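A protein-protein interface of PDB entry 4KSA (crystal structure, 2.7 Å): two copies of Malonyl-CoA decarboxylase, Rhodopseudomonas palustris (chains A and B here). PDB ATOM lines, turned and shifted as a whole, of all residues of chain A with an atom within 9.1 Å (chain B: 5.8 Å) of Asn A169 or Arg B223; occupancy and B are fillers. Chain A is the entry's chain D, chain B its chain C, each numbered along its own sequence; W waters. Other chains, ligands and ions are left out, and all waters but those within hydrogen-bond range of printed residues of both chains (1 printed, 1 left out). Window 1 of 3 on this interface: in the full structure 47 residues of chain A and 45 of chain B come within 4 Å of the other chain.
Water W1 bridges the side-chain hydroxyl (OG) of Ser B166 and the indole nitrogen (NE1) of Trp A167.
O of Trp A167 is in hydrogen-bond range of ND2 of Asn A169 (2.9 Å).
A ring nitrogen (NE2) of His A221 lies within hydrogen-bond range of the backbone carbonyl oxygen (O) of Asn A169 (2.8 Å).
A ring nitrogen (ND1) of His B221 sits close to the backbone NH of Arg B223 (3.2 Å).
NE2 of His B221 sits at hydrogen-bond distance from O of Asn B169, at 2.8 Å.
O of Trp B167 sits at hydrogen-bond distance from ND2 of Asn B169 (3.1 Å).
The backbone carbonyl oxygen of Trp A167 sits at hydrogen-bond distance from the guanidinium group of Arg A223.
Asn A169 touches Arg B223 (CG to NH1, 3.4 Å).
CZ of Phe A172 touches O of Pro B222, at 3.7 Å.
Phe A172 touches Arg B223.
NH1 of Arg A223 touches O of Ser B166, 3.97 Å away.
NH2 of Arg A223 sits at hydrogen-bond distance from OD1 of Asn B169 (3.5 Å).
OG of Ser B166 lies within hydrogen-bond range of OG of Ser A166.
Of the 21 printed residues of chain A, 4 touch a printed residue of chain B.
Hydrophobic or aromatic side chains of chain A within 4 Å of the printed part of chain B: Phe A172.
Among the printed residues, 6 pairs touch across the chains.
Among the printed residues, no Asp or Glu carboxylate lies within 4 Å of a Lys or Arg side-chain nitrogen of the other chain.
Of the printed residues of chain B, Ser A166 touches Ser B166 (2.8 Å).
Asn A169 touches just one residue of chain B: Arg B223 (3.4 Å).
Printed residues of chain B within 4 Å of Phe A172: Pro B222 and Arg B223.
His A221 touches none of the printed residues of chain B.
Gly A281 touches none of the printed residues of chain B.
Printed residues of chain A within 4 Å of Ser B166: Ser A166 (2.8 Å) and Arg A223 (3.97 Å).
Printed residues of chain A within 4 Å of Pro B222: Phe A172.
Arg B223 touches just these residues of chain A: Asn A169 (3.4 Å) and Phe A172 (3.5 Å).
Leu B224 touches none of the printed residues of chain A.
The nearest residue of chain A that does not touch Arg B223 is Ser A166 (4.1 Å).
The nearest printed residue of chain B that does not touch Ser A166 is Arg B223 (4.1 Å).
Ser A166 touches its own counterpart, Ser B166.
Asn A169 touches Arg B223, and with the chains exchanged Arg A223 touches Asn B169.
Arg A223 touches Ser B166, but with the chains exchanged Ser A166 does not touch Arg B223 (4.1 Å).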
ATOM      1  N   LEU A 163     -37.177  -2.307 -16.299  1.00  0.00           N
ATOM      2  CA  LEU A 163     -36.384  -2.278 -15.077  1.00  0.00           C
ATOM      3  C   LEU A 163     -35.471  -3.487 -15.005  1.00  0.00           C
ATOM      4  O   LEU A 163     -34.259  -3.335 -14.851  1.00  0.00           O
ATOM      5  CB  LEU A 163     -37.294  -2.236 -13.837  1.00  0.00           C
ATOM      6  CG  LEU A 163     -37.747  -0.861 -13.329  1.00  0.00           C
ATOM      7  CD1 LEU A 163     -37.322   0.229 -14.305  1.00  0.00           C
ATOM      8  CD2 LEU A 163     -39.261  -0.866 -13.119  1.00  0.00           C
ATOM      9  N   PHE A 164     -36.054  -4.680 -15.121  1.00  0.00           N
ATOM     10  CA  PHE A 164     -35.286  -5.917 -15.077  1.00  0.00           C
ATOM     11  C   PHE A 164     -34.104  -5.888 -16.038  1.00  0.00           C
ATOM     12  O   PHE A 164     -33.005  -6.333 -15.695  1.00  0.00           O
ATOM     13  CB  PHE A 164     -36.188  -7.101 -15.403  1.00  0.00           C
ATOM     14  CG  PHE A 164     -37.062  -7.513 -14.264  1.00  0.00           C
ATOM     15  CD1 PHE A 164     -37.911  -8.600 -14.385  1.00  0.00           C
ATOM     16  CD2 PHE A 164     -37.060  -6.796 -13.079  1.00  0.00           C
ATOM     17  CE1 PHE A 164     -38.753  -8.968 -13.348  1.00  0.00           C
ATOM     18  CE2 PHE A 164     -37.896  -7.150 -12.032  1.00  0.00           C
ATOM     19  CZ  PHE A 164     -38.748  -8.238 -12.165  1.00  0.00           C
ATOM     20  N   THR A 165     -34.324  -5.361 -17.236  1.00  0.00           N
ATOM     21  CA  THR A 165     -33.254  -5.290 -18.206  1.00  0.00           C
ATOM     22  C   THR A 165     -32.134  -4.437 -17.643  1.00  0.00           C
ATOM     23  O   THR A 165     -30.951  -4.695 -17.881  1.00  0.00           O
ATOM     24  CB  THR A 165     -33.744  -4.697 -19.524  1.00  0.00           C
ATOM     25  OG1 THR A 165     -34.809  -5.509 -20.035  1.00  0.00           O
ATOM     26  CG2 THR A 165     -32.629  -4.671 -20.546  1.00  0.00           C
ATOM     27  N   SER A 166     -32.491  -3.432 -16.865  1.00  0.00           N
ATOM     28  CA  SER A 166     -31.461  -2.595 -16.301  1.00  0.00           C
ATOM     29  C   SER A 166     -30.846  -3.196 -15.045  1.00  0.00           C
ATOM     30  O   SER A 166     -29.661  -3.058 -14.816  1.00  0.00           O
ATOM     31  CB  SER A 166     -32.001  -1.201 -16.012  1.00  0.00           C
ATOM     32  OG  SER A 166     -30.943  -0.368 -15.554  1.00  0.00           O
ATOM     33  N   TRP A 167     -31.642  -3.876 -14.236  1.00  0.00           N
ATOM     34  CA  TRP A 167     -31.132  -4.478 -13.003  1.00  0.00           C
ATOM     35  C   TRP A 167     -30.231  -5.701 -13.233  1.00  0.00           C
ATOM     36  O   TRP A 167     -29.157  -5.829 -12.632  1.00  0.00           O
ATOM     37  CB  TRP A 167     -32.303  -4.858 -12.100  1.00  0.00           C
ATOM     38  CG  TRP A 167     -33.081  -3.664 -11.643  1.00  0.00           C
ATOM     39  CD1 TRP A 167     -32.707  -2.347 -11.752  1.00  0.00           C
ATOM     40  CD2 TRP A 167     -34.334  -3.668 -10.947  1.00  0.00           C
ATOM     41  NE1 TRP A 167     -33.656  -1.532 -11.165  1.00  0.00           N
ATOM     42  CE2 TRP A 167     -34.665  -2.320 -10.670  1.00  0.00           C
ATOM     43  CE3 TRP A 167     -35.217  -4.675 -10.543  1.00  0.00           C
ATOM     44  CZ2 TRP A 167     -35.826  -1.966  -9.989  1.00  0.00           C
ATOM     45  CZ3 TRP A 167     -36.369  -4.319  -9.871  1.00  0.00           C
ATOM     46  CH2 TRP A 167     -36.667  -2.978  -9.609  1.00  0.00           C
ATOM     47  N   PHE A 168     -30.676  -6.591 -14.112  1.00  0.00           N
ATOM     48  CA  PHE A 168     -29.914  -7.784 -14.424  1.00  0.00           C
ATOM     49  C   PHE A 168     -28.851  -7.524 -15.499  1.00  0.00           C
ATOM     50  O   PHE A 168     -28.909  -8.079 -16.596  1.00  0.00           O
ATOM     51  CB  PHE A 168     -30.875  -8.910 -14.838  1.00  0.00           C
ATOM     52  CG  PHE A 168     -31.686  -9.445 -13.693  1.00  0.00           C
ATOM     53  CD1 PHE A 168     -32.913  -8.881 -13.365  1.00  0.00           C
ATOM     54  CD2 PHE A 168     -31.177 -10.458 -12.874  1.00  0.00           C
ATOM     55  CE1 PHE A 168     -33.615  -9.309 -12.239  1.00  0.00           C
ATOM     56  CE2 PHE A 168     -31.872 -10.895 -11.743  1.00  0.00           C
ATOM     57  CZ  PHE A 168     -33.085 -10.325 -11.423  1.00  0.00           C
ATOM     58  N   ASN A 169     -27.881  -6.675 -15.187  1.00  0.00           N
ATOM     59  CA  ASN A 169     -26.827  -6.380 -16.139  1.00  0.00           C
ATOM     60  C   ASN A 169     -25.977  -7.623 -16.346  1.00  0.00           C
ATOM     61  O   ASN A 169     -25.657  -8.328 -15.394  1.00  0.00           O
ATOM     62  CB  ASN A 169     -25.955  -5.218 -15.641  1.00  0.00           C
ATOM     63  CG  ASN A 169     -25.412  -5.438 -14.234  1.00  0.00           C
ATOM     64  OD1 ASN A 169     -24.212  -5.276 -13.984  1.00  0.00           O
ATOM     65  ND2 ASN A 169     -26.299  -5.796 -13.303  1.00  0.00           N
ATOM     66  N   ARG A 170     -25.613  -7.900 -17.590  1.00  0.00           N
ATOM     67  CA  ARG A 170     -24.809  -9.080 -17.875  1.00  0.00           C
ATOM     68  C   ARG A 170     -23.384  -8.984 -17.319  1.00  0.00           C
ATOM     69  O   ARG A 170     -22.691  -9.994 -17.155  1.00  0.00           O
ATOM     70  CB  ARG A 170     -24.806  -9.366 -19.384  1.00  0.00           C
ATOM     71  CG  ARG A 170     -24.611  -8.169 -20.292  1.00  0.00           C
ATOM     72  CD  ARG A 170     -25.420  -8.367 -21.593  1.00  0.00           C
ATOM     73  NE  ARG A 170     -24.960  -7.520 -22.700  1.00  0.00           N
ATOM     74  CZ  ARG A 170     -23.740  -7.581 -23.234  1.00  0.00           C
ATOM     75  NH1 ARG A 170     -22.856  -8.451 -22.759  1.00  0.00           N
ATOM     76  NH2 ARG A 170     -23.398  -6.773 -24.232  1.00  0.00           N
ATOM     77  N   GLY A 171     -22.964  -7.768 -16.998  1.00  0.00           N
ATOM     78  CA  GLY A 171     -21.639  -7.566 -16.448  1.00  0.00           C
ATOM     79  C   GLY A 171     -21.428  -8.243 -15.101  1.00  0.00           C
ATOM     80  O   GLY A 171     -20.281  -8.564 -14.759  1.00  0.00           O
ATOM     81  N   PHE A 172     -22.503  -8.447 -14.328  1.00  0.00           N
ATOM     82  CA  PHE A 172     -22.379  -9.101 -13.021  1.00  0.00           C
ATOM     83  C   PHE A 172     -22.824 -10.555 -13.058  1.00  0.00           C
ATOM     84  O   PHE A 172     -22.978 -11.189 -12.029  1.00  0.00           O
ATOM     85  CB  PHE A 172     -23.169  -8.370 -11.922  1.00  0.00           C
ATOM     86  CG  PHE A 172     -22.673  -6.978 -11.627  1.00  0.00           C
ATOM     87  CD1 PHE A 172     -21.392  -6.579 -11.995  1.00  0.00           C
ATOM     88  CD2 PHE A 172     -23.501  -6.055 -10.994  1.00  0.00           C
ATOM     89  CE1 PHE A 172     -20.948  -5.285 -11.744  1.00  0.00           C
ATOM     90  CE2 PHE A 172     -23.068  -4.757 -10.738  1.00  0.00           C
ATOM     91  CZ  PHE A 172     -21.789  -4.368 -11.113  1.00  0.00           C
ATOM     92  N   LEU A 173     -23.046 -11.088 -14.248  1.00  0.00           N
ATOM     93  CA  LEU A 173     -23.435 -12.479 -14.356  1.00  0.00           C
ATOM     94  C   LEU A 173     -22.158 -13.275 -14.044  1.00  0.00           C
ATOM     95  O   LEU A 173     -21.104 -13.042 -14.630  1.00  0.00           O
ATOM     96  CB  LEU A 173     -23.939 -12.743 -15.764  1.00  0.00           C
ATOM     97  CG  LEU A 173     -24.812 -13.980 -15.882  1.00  0.00           C
ATOM     98  CD1 LEU A 173     -25.978 -13.922 -14.897  1.00  0.00           C
ATOM     99  CD2 LEU A 173     -25.287 -14.069 -17.310  1.00  0.00           C
ATOM    100  N   VAL A 174     -22.238 -14.208 -13.114  1.00  0.00           N
ATOM    101  CA  VAL A 174     -21.040 -14.943 -12.739  1.00  0.00           C
ATOM    102  C   VAL A 174     -21.163 -16.440 -12.913  1.00  0.00           C
ATOM    103  O   VAL A 174     -22.123 -17.054 -12.429  1.00  0.00           O
ATOM    104  CB  VAL A 174     -20.655 -14.643 -11.254  1.00  0.00           C
ATOM    105  CG1 VAL A 174     -19.543 -15.570 -10.788  1.00  0.00           C
ATOM    106  CG2 VAL A 174     -20.225 -13.182 -11.114  1.00  0.00           C
ATOM    107  N   PHE A 220     -24.814 -16.976 -11.889  1.00  0.00           N
ATOM    108  CA  PHE A 220     -25.473 -16.328 -10.762  1.00  0.00           C
ATOM    109  C   PHE A 220     -25.370 -14.809 -10.907  1.00  0.00           C
ATOM    110  O   PHE A 220     -24.436 -14.301 -11.533  1.00  0.00           O
ATOM    111  CB  PHE A 220     -24.827 -16.776  -9.446  1.00  0.00           C
ATOM    112  CG  PHE A 220     -24.964 -18.254  -9.165  1.00  0.00           C
ATOM    113  CD1 PHE A 220     -25.935 -18.723  -8.277  1.00  0.00           C
ATOM    114  CD2 PHE A 220     -24.144 -19.180  -9.798  1.00  0.00           C
ATOM    115  CE1 PHE A 220     -26.093 -20.098  -8.023  1.00  0.00           C
ATOM    116  CE2 PHE A 220     -24.298 -20.552  -9.551  1.00  0.00           C
ATOM    117  CZ  PHE A 220     -25.283 -21.007  -8.656  1.00  0.00           C
ATOM    118  N   HIS A 221     -26.339 -14.099 -10.333  1.00  0.00           N
ATOM    119  CA  HIS A 221     -26.380 -12.640 -10.378  1.00  0.00           C
ATOM    120  C   HIS A 221     -26.638 -12.107  -8.971  1.00  0.00           C
ATOM    121  O   HIS A 221     -27.469 -12.644  -8.240  1.00  0.00           O
ATOM    122  CB  HIS A 221     -27.486 -12.177 -11.326  1.00  0.00           C
ATOM    123  CG  HIS A 221     -27.282 -10.790 -11.836  1.00  0.00           C
ATOM    124  ND1 HIS A 221     -27.512  -9.672 -11.064  1.00  0.00           N
ATOM    125  CD2 HIS A 221     -26.761 -10.342 -13.002  1.00  0.00           C
ATOM    126  CE1 HIS A 221     -27.131  -8.597 -11.731  1.00  0.00           C
ATOM    127  NE2 HIS A 221     -26.669  -8.976 -12.909  1.00  0.00           N
ATOM    128  N   PRO A 222     -25.926 -11.053  -8.566  1.00  0.00           N
ATOM    129  CA  PRO A 222     -26.140 -10.518  -7.223  1.00  0.00           C
ATOM    130  C   PRO A 222     -27.559 -10.046  -6.918  1.00  0.00           C
ATOM    131  O   PRO A 222     -27.894  -9.791  -5.772  1.00  0.00           O
ATOM    132  CB  PRO A 222     -25.097  -9.400  -7.115  1.00  0.00           C
ATOM    133  CG  PRO A 222     -24.809  -9.029  -8.527  1.00  0.00           C
ATOM    134  CD  PRO A 222     -24.845 -10.337  -9.256  1.00  0.00           C
ATOM    135  N   ARG A 223     -28.394  -9.939  -7.942  1.00  0.00           N
ATOM    136  CA  ARG A 223     -29.765  -9.510  -7.748  1.00  0.00           C
ATOM    137  C   ARG A 223     -30.616 -10.589  -7.117  1.00  0.00           C
ATOM    138  O   ARG A 223     -31.561 -10.261  -6.399  1.00  0.00           O
ATOM    139  CB  ARG A 223     -30.376  -9.093  -9.070  1.00  0.00           C
ATOM    140  CG  ARG A 223     -29.771  -7.831  -9.638  1.00  0.00           C
ATOM    141  CD  ARG A 223     -30.208  -6.598  -8.866  1.00  0.00           C
ATOM    142  NE  ARG A 223     -29.745  -5.386  -9.540  1.00  0.00           N
ATOM    143  CZ  ARG A 223     -30.087  -4.152  -9.187  1.00  0.00           C
ATOM    144  NH1 ARG A 223     -29.618  -3.120  -9.868  1.00  0.00           N
ATOM    145  NH2 ARG A 223     -30.892  -3.955  -8.150  1.00  0.00           N
ATOM    146  N   LEU A 229     -29.497 -18.505 -12.344  1.00  0.00           N
ATOM    147  CA  LEU A 229     -30.318 -17.999 -13.432  1.00  0.00           C
ATOM    148  C   LEU A 229     -30.331 -18.954 -14.616  1.00  0.00           C
ATOM    149  O   LEU A 229     -31.389 -19.252 -15.189  1.00  0.00           O
ATOM    150  CB  LEU A 229     -29.812 -16.628 -13.860  1.00  0.00           C
ATOM    151  CG  LEU A 229     -30.363 -15.451 -13.052  1.00  0.00           C
ATOM    152  CD1 LEU A 229     -30.333 -15.749 -11.565  1.00  0.00           C
ATOM    153  CD2 LEU A 229     -29.572 -14.200 -13.388  1.00  0.00           C
ATOM    154  N   ILE A 278     -35.456 -11.676 -20.814  1.00  0.00           N
ATOM    155  CA  ILE A 278     -34.365 -10.797 -20.457  1.00  0.00           C
ATOM    156  C   ILE A 278     -33.108 -11.484 -20.936  1.00  0.00           C
ATOM    157  O   ILE A 278     -32.794 -12.593 -20.510  1.00  0.00           O
ATOM    158  CB  ILE A 278     -34.266 -10.563 -18.956  1.00  0.00           C
ATOM    159  CG1 ILE A 278     -35.408  -9.660 -18.493  1.00  0.00           C
ATOM    160  CG2 ILE A 278     -32.952  -9.917 -18.637  1.00  0.00           C
ATOM    161  CD1 ILE A 278     -36.763 -10.326 -18.551  1.00  0.00           C
ATOM    162  N   SER A 279     -32.393 -10.835 -21.836  1.00  0.00           N
ATOM    163  CA  SER A 279     -31.176 -11.420 -22.366  1.00  0.00           C
ATOM    164  C   SER A 279     -30.057 -11.321 -21.336  1.00  0.00           C
ATOM    165  O   SER A 279     -29.881 -10.275 -20.708  1.00  0.00           O
ATOM    166  CB  SER A 279     -30.763 -10.705 -23.666  1.00  0.00           C
ATOM    167  OG  SER A 279     -29.579 -11.267 -24.219  1.00  0.00           O
ATOM    168  N   PHE A 280     -29.320 -12.418 -21.162  1.00  0.00           N
ATOM    169  CA  PHE A 280     -28.192 -12.457 -20.237  1.00  0.00           C
ATOM    170  C   PHE A 280     -26.915 -12.437 -21.063  1.00  0.00           C
ATOM    171  O   PHE A 280     -25.832 -12.664 -20.535  1.00  0.00           O
ATOM    172  CB  PHE A 280     -28.192 -13.731 -19.391  1.00  0.00           C
ATOM    173  CG  PHE A 280     -29.447 -13.943 -18.602  1.00  0.00           C
ATOM    174  CD1 PHE A 280     -29.897 -12.978 -17.712  1.00  0.00           C
ATOM    175  CD2 PHE A 280     -30.167 -15.128 -18.726  1.00  0.00           C
ATOM    176  CE1 PHE A 280     -31.054 -13.194 -16.953  1.00  0.00           C
ATOM    177  CE2 PHE A 280     -31.317 -15.354 -17.973  1.00  0.00           C
ATOM    178  CZ  PHE A 280     -31.763 -14.386 -17.085  1.00  0.00           C
ATOM    179  N   GLY A 281     -27.044 -12.179 -22.361  1.00  0.00           N
ATOM    180  CA  GLY A 281     -25.872 -12.141 -23.219  1.00  0.00           C
ATOM    181  C   GLY A 281     -25.839 -13.313 -24.180  1.00  0.00           C
ATOM    182  O   GLY A 281     -26.498 -14.341 -23.961  1.00  0.00           O
ATOM    183  N   ASN B 127     -21.447   1.349 -21.906  1.00  0.00           N
ATOM    184  CA  ASN B 127     -21.206   0.715 -20.633  1.00  0.00           C
ATOM    185  C   ASN B 127     -20.861  -0.759 -20.715  1.00  0.00           C
ATOM    186  O   ASN B 127     -20.483  -1.357 -19.716  1.00  0.00           O
ATOM    187  CB  ASN B 127     -22.403   0.943 -19.716  1.00  0.00           C
ATOM    188  CG  ASN B 127     -22.062   0.725 -18.248  1.00  0.00           C
ATOM    189  OD1 ASN B 127     -20.987   1.097 -17.789  1.00  0.00           O
ATOM    190  ND2 ASN B 127     -22.983   0.144 -17.508  1.00  0.00           N
ATOM    191  N   THR B 133     -17.915   1.771 -17.346  1.00  0.00           N
ATOM    192  CA  THR B 133     -18.507   2.557 -16.293  1.00  0.00           C
ATOM    193  C   THR B 133     -17.569   3.609 -15.748  1.00  0.00           C
ATOM    194  O   THR B 133     -17.966   4.747 -15.514  1.00  0.00           O
ATOM    195  CB  THR B 133     -18.950   1.695 -15.184  1.00  0.00           C
ATOM    196  OG1 THR B 133     -19.837   0.716 -15.707  1.00  0.00           O
ATOM    197  CG2 THR B 133     -19.701   2.519 -14.150  1.00  0.00           C
ATOM    198  N   ALA B 134     -16.317   3.230 -15.556  1.00  0.00           N
ATOM    199  CA  ALA B 134     -15.333   4.158 -15.033  1.00  0.00           C
ATOM    200  C   ALA B 134     -15.124   5.293 -16.008  1.00  0.00           C
ATOM    201  O   ALA B 134     -14.980   6.435 -15.601  1.00  0.00           O
ATOM    202  CB  ALA B 134     -14.013   3.441 -14.763  1.00  0.00           C
ATOM    203  N   SER B 166     -29.751   4.125 -11.572  1.00  0.00           N
ATOM    204  CA  SER B 166     -30.176   2.752 -11.697  1.00  0.00           C
ATOM    205  C   SER B 166     -29.040   1.755 -11.486  1.00  0.00           C
ATOM    206  O   SER B 166     -29.251   0.689 -10.923  1.00  0.00           O
ATOM    207  CB  SER B 166     -30.800   2.524 -13.066  1.00  0.00           C
ATOM    208  OG  SER B 166     -31.209   1.170 -13.196  1.00  0.00           O
ATOM    209  N   TRP B 167     -27.838   2.092 -11.940  1.00  0.00           N
ATOM    210  CA  TRP B 167     -26.707   1.176 -11.806  1.00  0.00           C
ATOM    211  C   TRP B 167     -26.207   1.114 -10.379  1.00  0.00           C
ATOM    212  O   TRP B 167     -26.116   0.038  -9.791  1.00  0.00           O
ATOM    213  CB  TRP B 167     -25.550   1.564 -12.750  1.00  0.00           C
ATOM    214  CG  TRP B 167     -25.953   1.591 -14.186  1.00  0.00           C
ATOM    215  CD1 TRP B 167     -27.052   1.001 -14.735  1.00  0.00           C
ATOM    216  CD2 TRP B 167     -25.297   2.282 -15.254  1.00  0.00           C
ATOM    217  NE1 TRP B 167     -27.127   1.286 -16.077  1.00  0.00           N
ATOM    218  CE2 TRP B 167     -26.059   2.070 -16.420  1.00  0.00           C
ATOM    219  CE3 TRP B 167     -24.138   3.064 -15.340  1.00  0.00           C
ATOM    220  CZ2 TRP B 167     -25.701   2.614 -17.656  1.00  0.00           C
ATOM    221  CZ3 TRP B 167     -23.784   3.607 -16.575  1.00  0.00           C
ATOM    222  CH2 TRP B 167     -24.562   3.377 -17.711  1.00  0.00           C
ATOM    223  N   PHE B 168     -25.889   2.271  -9.818  1.00  0.00           N
ATOM    224  CA  PHE B 168     -25.400   2.322  -8.454  1.00  0.00           C
ATOM    225  C   PHE B 168     -26.477   2.104  -7.398  1.00  0.00           C
ATOM    226  O   PHE B 168     -26.713   2.972  -6.564  1.00  0.00           O
ATOM    227  CB  PHE B 168     -24.688   3.646  -8.222  1.00  0.00           C
ATOM    228  CG  PHE B 168     -23.475   3.815  -9.066  1.00  0.00           C
ATOM    229  CD1 PHE B 168     -23.560   4.414 -10.316  1.00  0.00           C
ATOM    230  CD2 PHE B 168     -22.245   3.333  -8.638  1.00  0.00           C
ATOM    231  CE1 PHE B 168     -22.427   4.527 -11.134  1.00  0.00           C
ATOM    232  CE2 PHE B 168     -21.112   3.440  -9.441  1.00  0.00           C
ATOM    233  CZ  PHE B 168     -21.203   4.037 -10.691  1.00  0.00           C
ATOM    234  N   ASN B 169     -27.130   0.944  -7.443  1.00  0.00           N
ATOM    235  CA  ASN B 169     -28.167   0.611  -6.474  1.00  0.00           C
ATOM    236  C   ASN B 169     -27.547   0.536  -5.074  1.00  0.00           C
ATOM    237  O   ASN B 169     -26.490  -0.080  -4.893  1.00  0.00           O
ATOM    238  CB  ASN B 169     -28.805  -0.724  -6.828  1.00  0.00           C
ATOM    239  CG  ASN B 169     -27.823  -1.867  -6.760  1.00  0.00           C
ATOM    240  OD1 ASN B 169     -28.139  -2.936  -6.250  1.00  0.00           O
ATOM    241  ND2 ASN B 169     -26.628  -1.655  -7.284  1.00  0.00           N
ATOM    242  N   HIS B 221     -18.694  -0.029  -4.292  1.00  0.00           N
ATOM    243  CA  HIS B 221     -19.795  -0.545  -5.095  1.00  0.00           C
ATOM    244  C   HIS B 221     -19.215  -1.390  -6.241  1.00  0.00           C
ATOM    245  O   HIS B 221     -18.211  -1.017  -6.853  1.00  0.00           O
ATOM    246  CB  HIS B 221     -20.632   0.606  -5.648  1.00  0.00           C
ATOM    247  CG  HIS B 221     -21.991   0.187  -6.111  1.00  0.00           C
ATOM    248  ND1 HIS B 221     -22.209  -0.435  -7.323  1.00  0.00           N
ATOM    249  CD2 HIS B 221     -23.195   0.248  -5.494  1.00  0.00           C
ATOM    250  CE1 HIS B 221     -23.491  -0.737  -7.430  1.00  0.00           C
ATOM    251  NE2 HIS B 221     -24.111  -0.334  -6.334  1.00  0.00           N
ATOM    252  N   PRO B 222     -19.825  -2.549  -6.527  1.00  0.00           N
ATOM    253  CA  PRO B 222     -19.325  -3.403  -7.604  1.00  0.00           C
ATOM    254  C   PRO B 222     -19.245  -2.755  -8.990  1.00  0.00           C
ATOM    255  O   PRO B 222     -18.520  -3.249  -9.856  1.00  0.00           O
ATOM    256  CB  PRO B 222     -20.268  -4.606  -7.561  1.00  0.00           C
ATOM    257  CG  PRO B 222     -21.509  -4.072  -6.918  1.00  0.00           C
ATOM    258  CD  PRO B 222     -20.962  -3.185  -5.843  1.00  0.00           C
ATOM    259  N   ARG B 223     -19.971  -1.657  -9.214  1.00  0.00           N
ATOM    260  CA  ARG B 223     -19.913  -0.994 -10.517  1.00  0.00           C
ATOM    261  C   ARG B 223     -18.545  -0.381 -10.743  1.00  0.00           C
ATOM    262  O   ARG B 223     -18.150  -0.175 -11.890  1.00  0.00           O
ATOM    263  CB  ARG B 223     -20.975   0.102 -10.656  1.00  0.00           C
ATOM    264  CG  ARG B 223     -22.401  -0.381 -10.773  1.00  0.00           C
ATOM    265  CD  ARG B 223     -22.670  -1.107 -12.077  1.00  0.00           C
ATOM    266  NE  ARG B 223     -24.061  -1.560 -12.147  1.00  0.00           N
ATOM    267  CZ  ARG B 223     -24.720  -1.783 -13.282  1.00  0.00           C
ATOM    268  NH1 ARG B 223     -25.989  -2.188 -13.243  1.00  0.00           N
ATOM    269  NH2 ARG B 223     -24.116  -1.596 -14.453  1.00  0.00           N
ATOM    270  N   LEU B 224     -17.833  -0.067  -9.665  1.00  0.00           N
ATOM    271  CA  LEU B 224     -16.480   0.501  -9.777  1.00  0.00           C
ATOM    272  C   LEU B 224     -15.551  -0.223  -8.807  1.00  0.00           C
ATOM    273  O   LEU B 224     -15.473   0.119  -7.637  1.00  0.00           O
ATOM    274  CB  LEU B 224     -16.480   2.000  -9.471  1.00  0.00           C
ATOM    275  CG  LEU B 224     -17.195   2.952 -10.431  1.00  0.00           C
ATOM    276  CD1 LEU B 224     -17.189   4.351  -9.822  1.00  0.00           C
ATOM    277  CD2 LEU B 224     -16.518   2.948 -11.793  1.00  0.00           C
ATOM    278  N   VAL B 225     -14.849  -1.222  -9.316  1.00  0.00           N
ATOM    279  CA  VAL B 225     -13.956  -2.050  -8.529  1.00  0.00           C
ATOM    280  C   VAL B 225     -12.788  -1.349  -7.852  1.00  0.00           C
ATOM    281  O   VAL B 225     -12.097  -0.529  -8.457  1.00  0.00           O
ATOM    282  CB  VAL B 225     -13.431  -3.215  -9.408  1.00  0.00           C
ATOM    283  CG1 VAL B 225     -12.360  -4.022  -8.673  1.00  0.00           C
ATOM    284  CG2 VAL B 225     -14.609  -4.122  -9.780  1.00  0.00           C
HETATM  285  O   HOH W   1     -34.011   1.665 -11.863  1.00  0.00           O
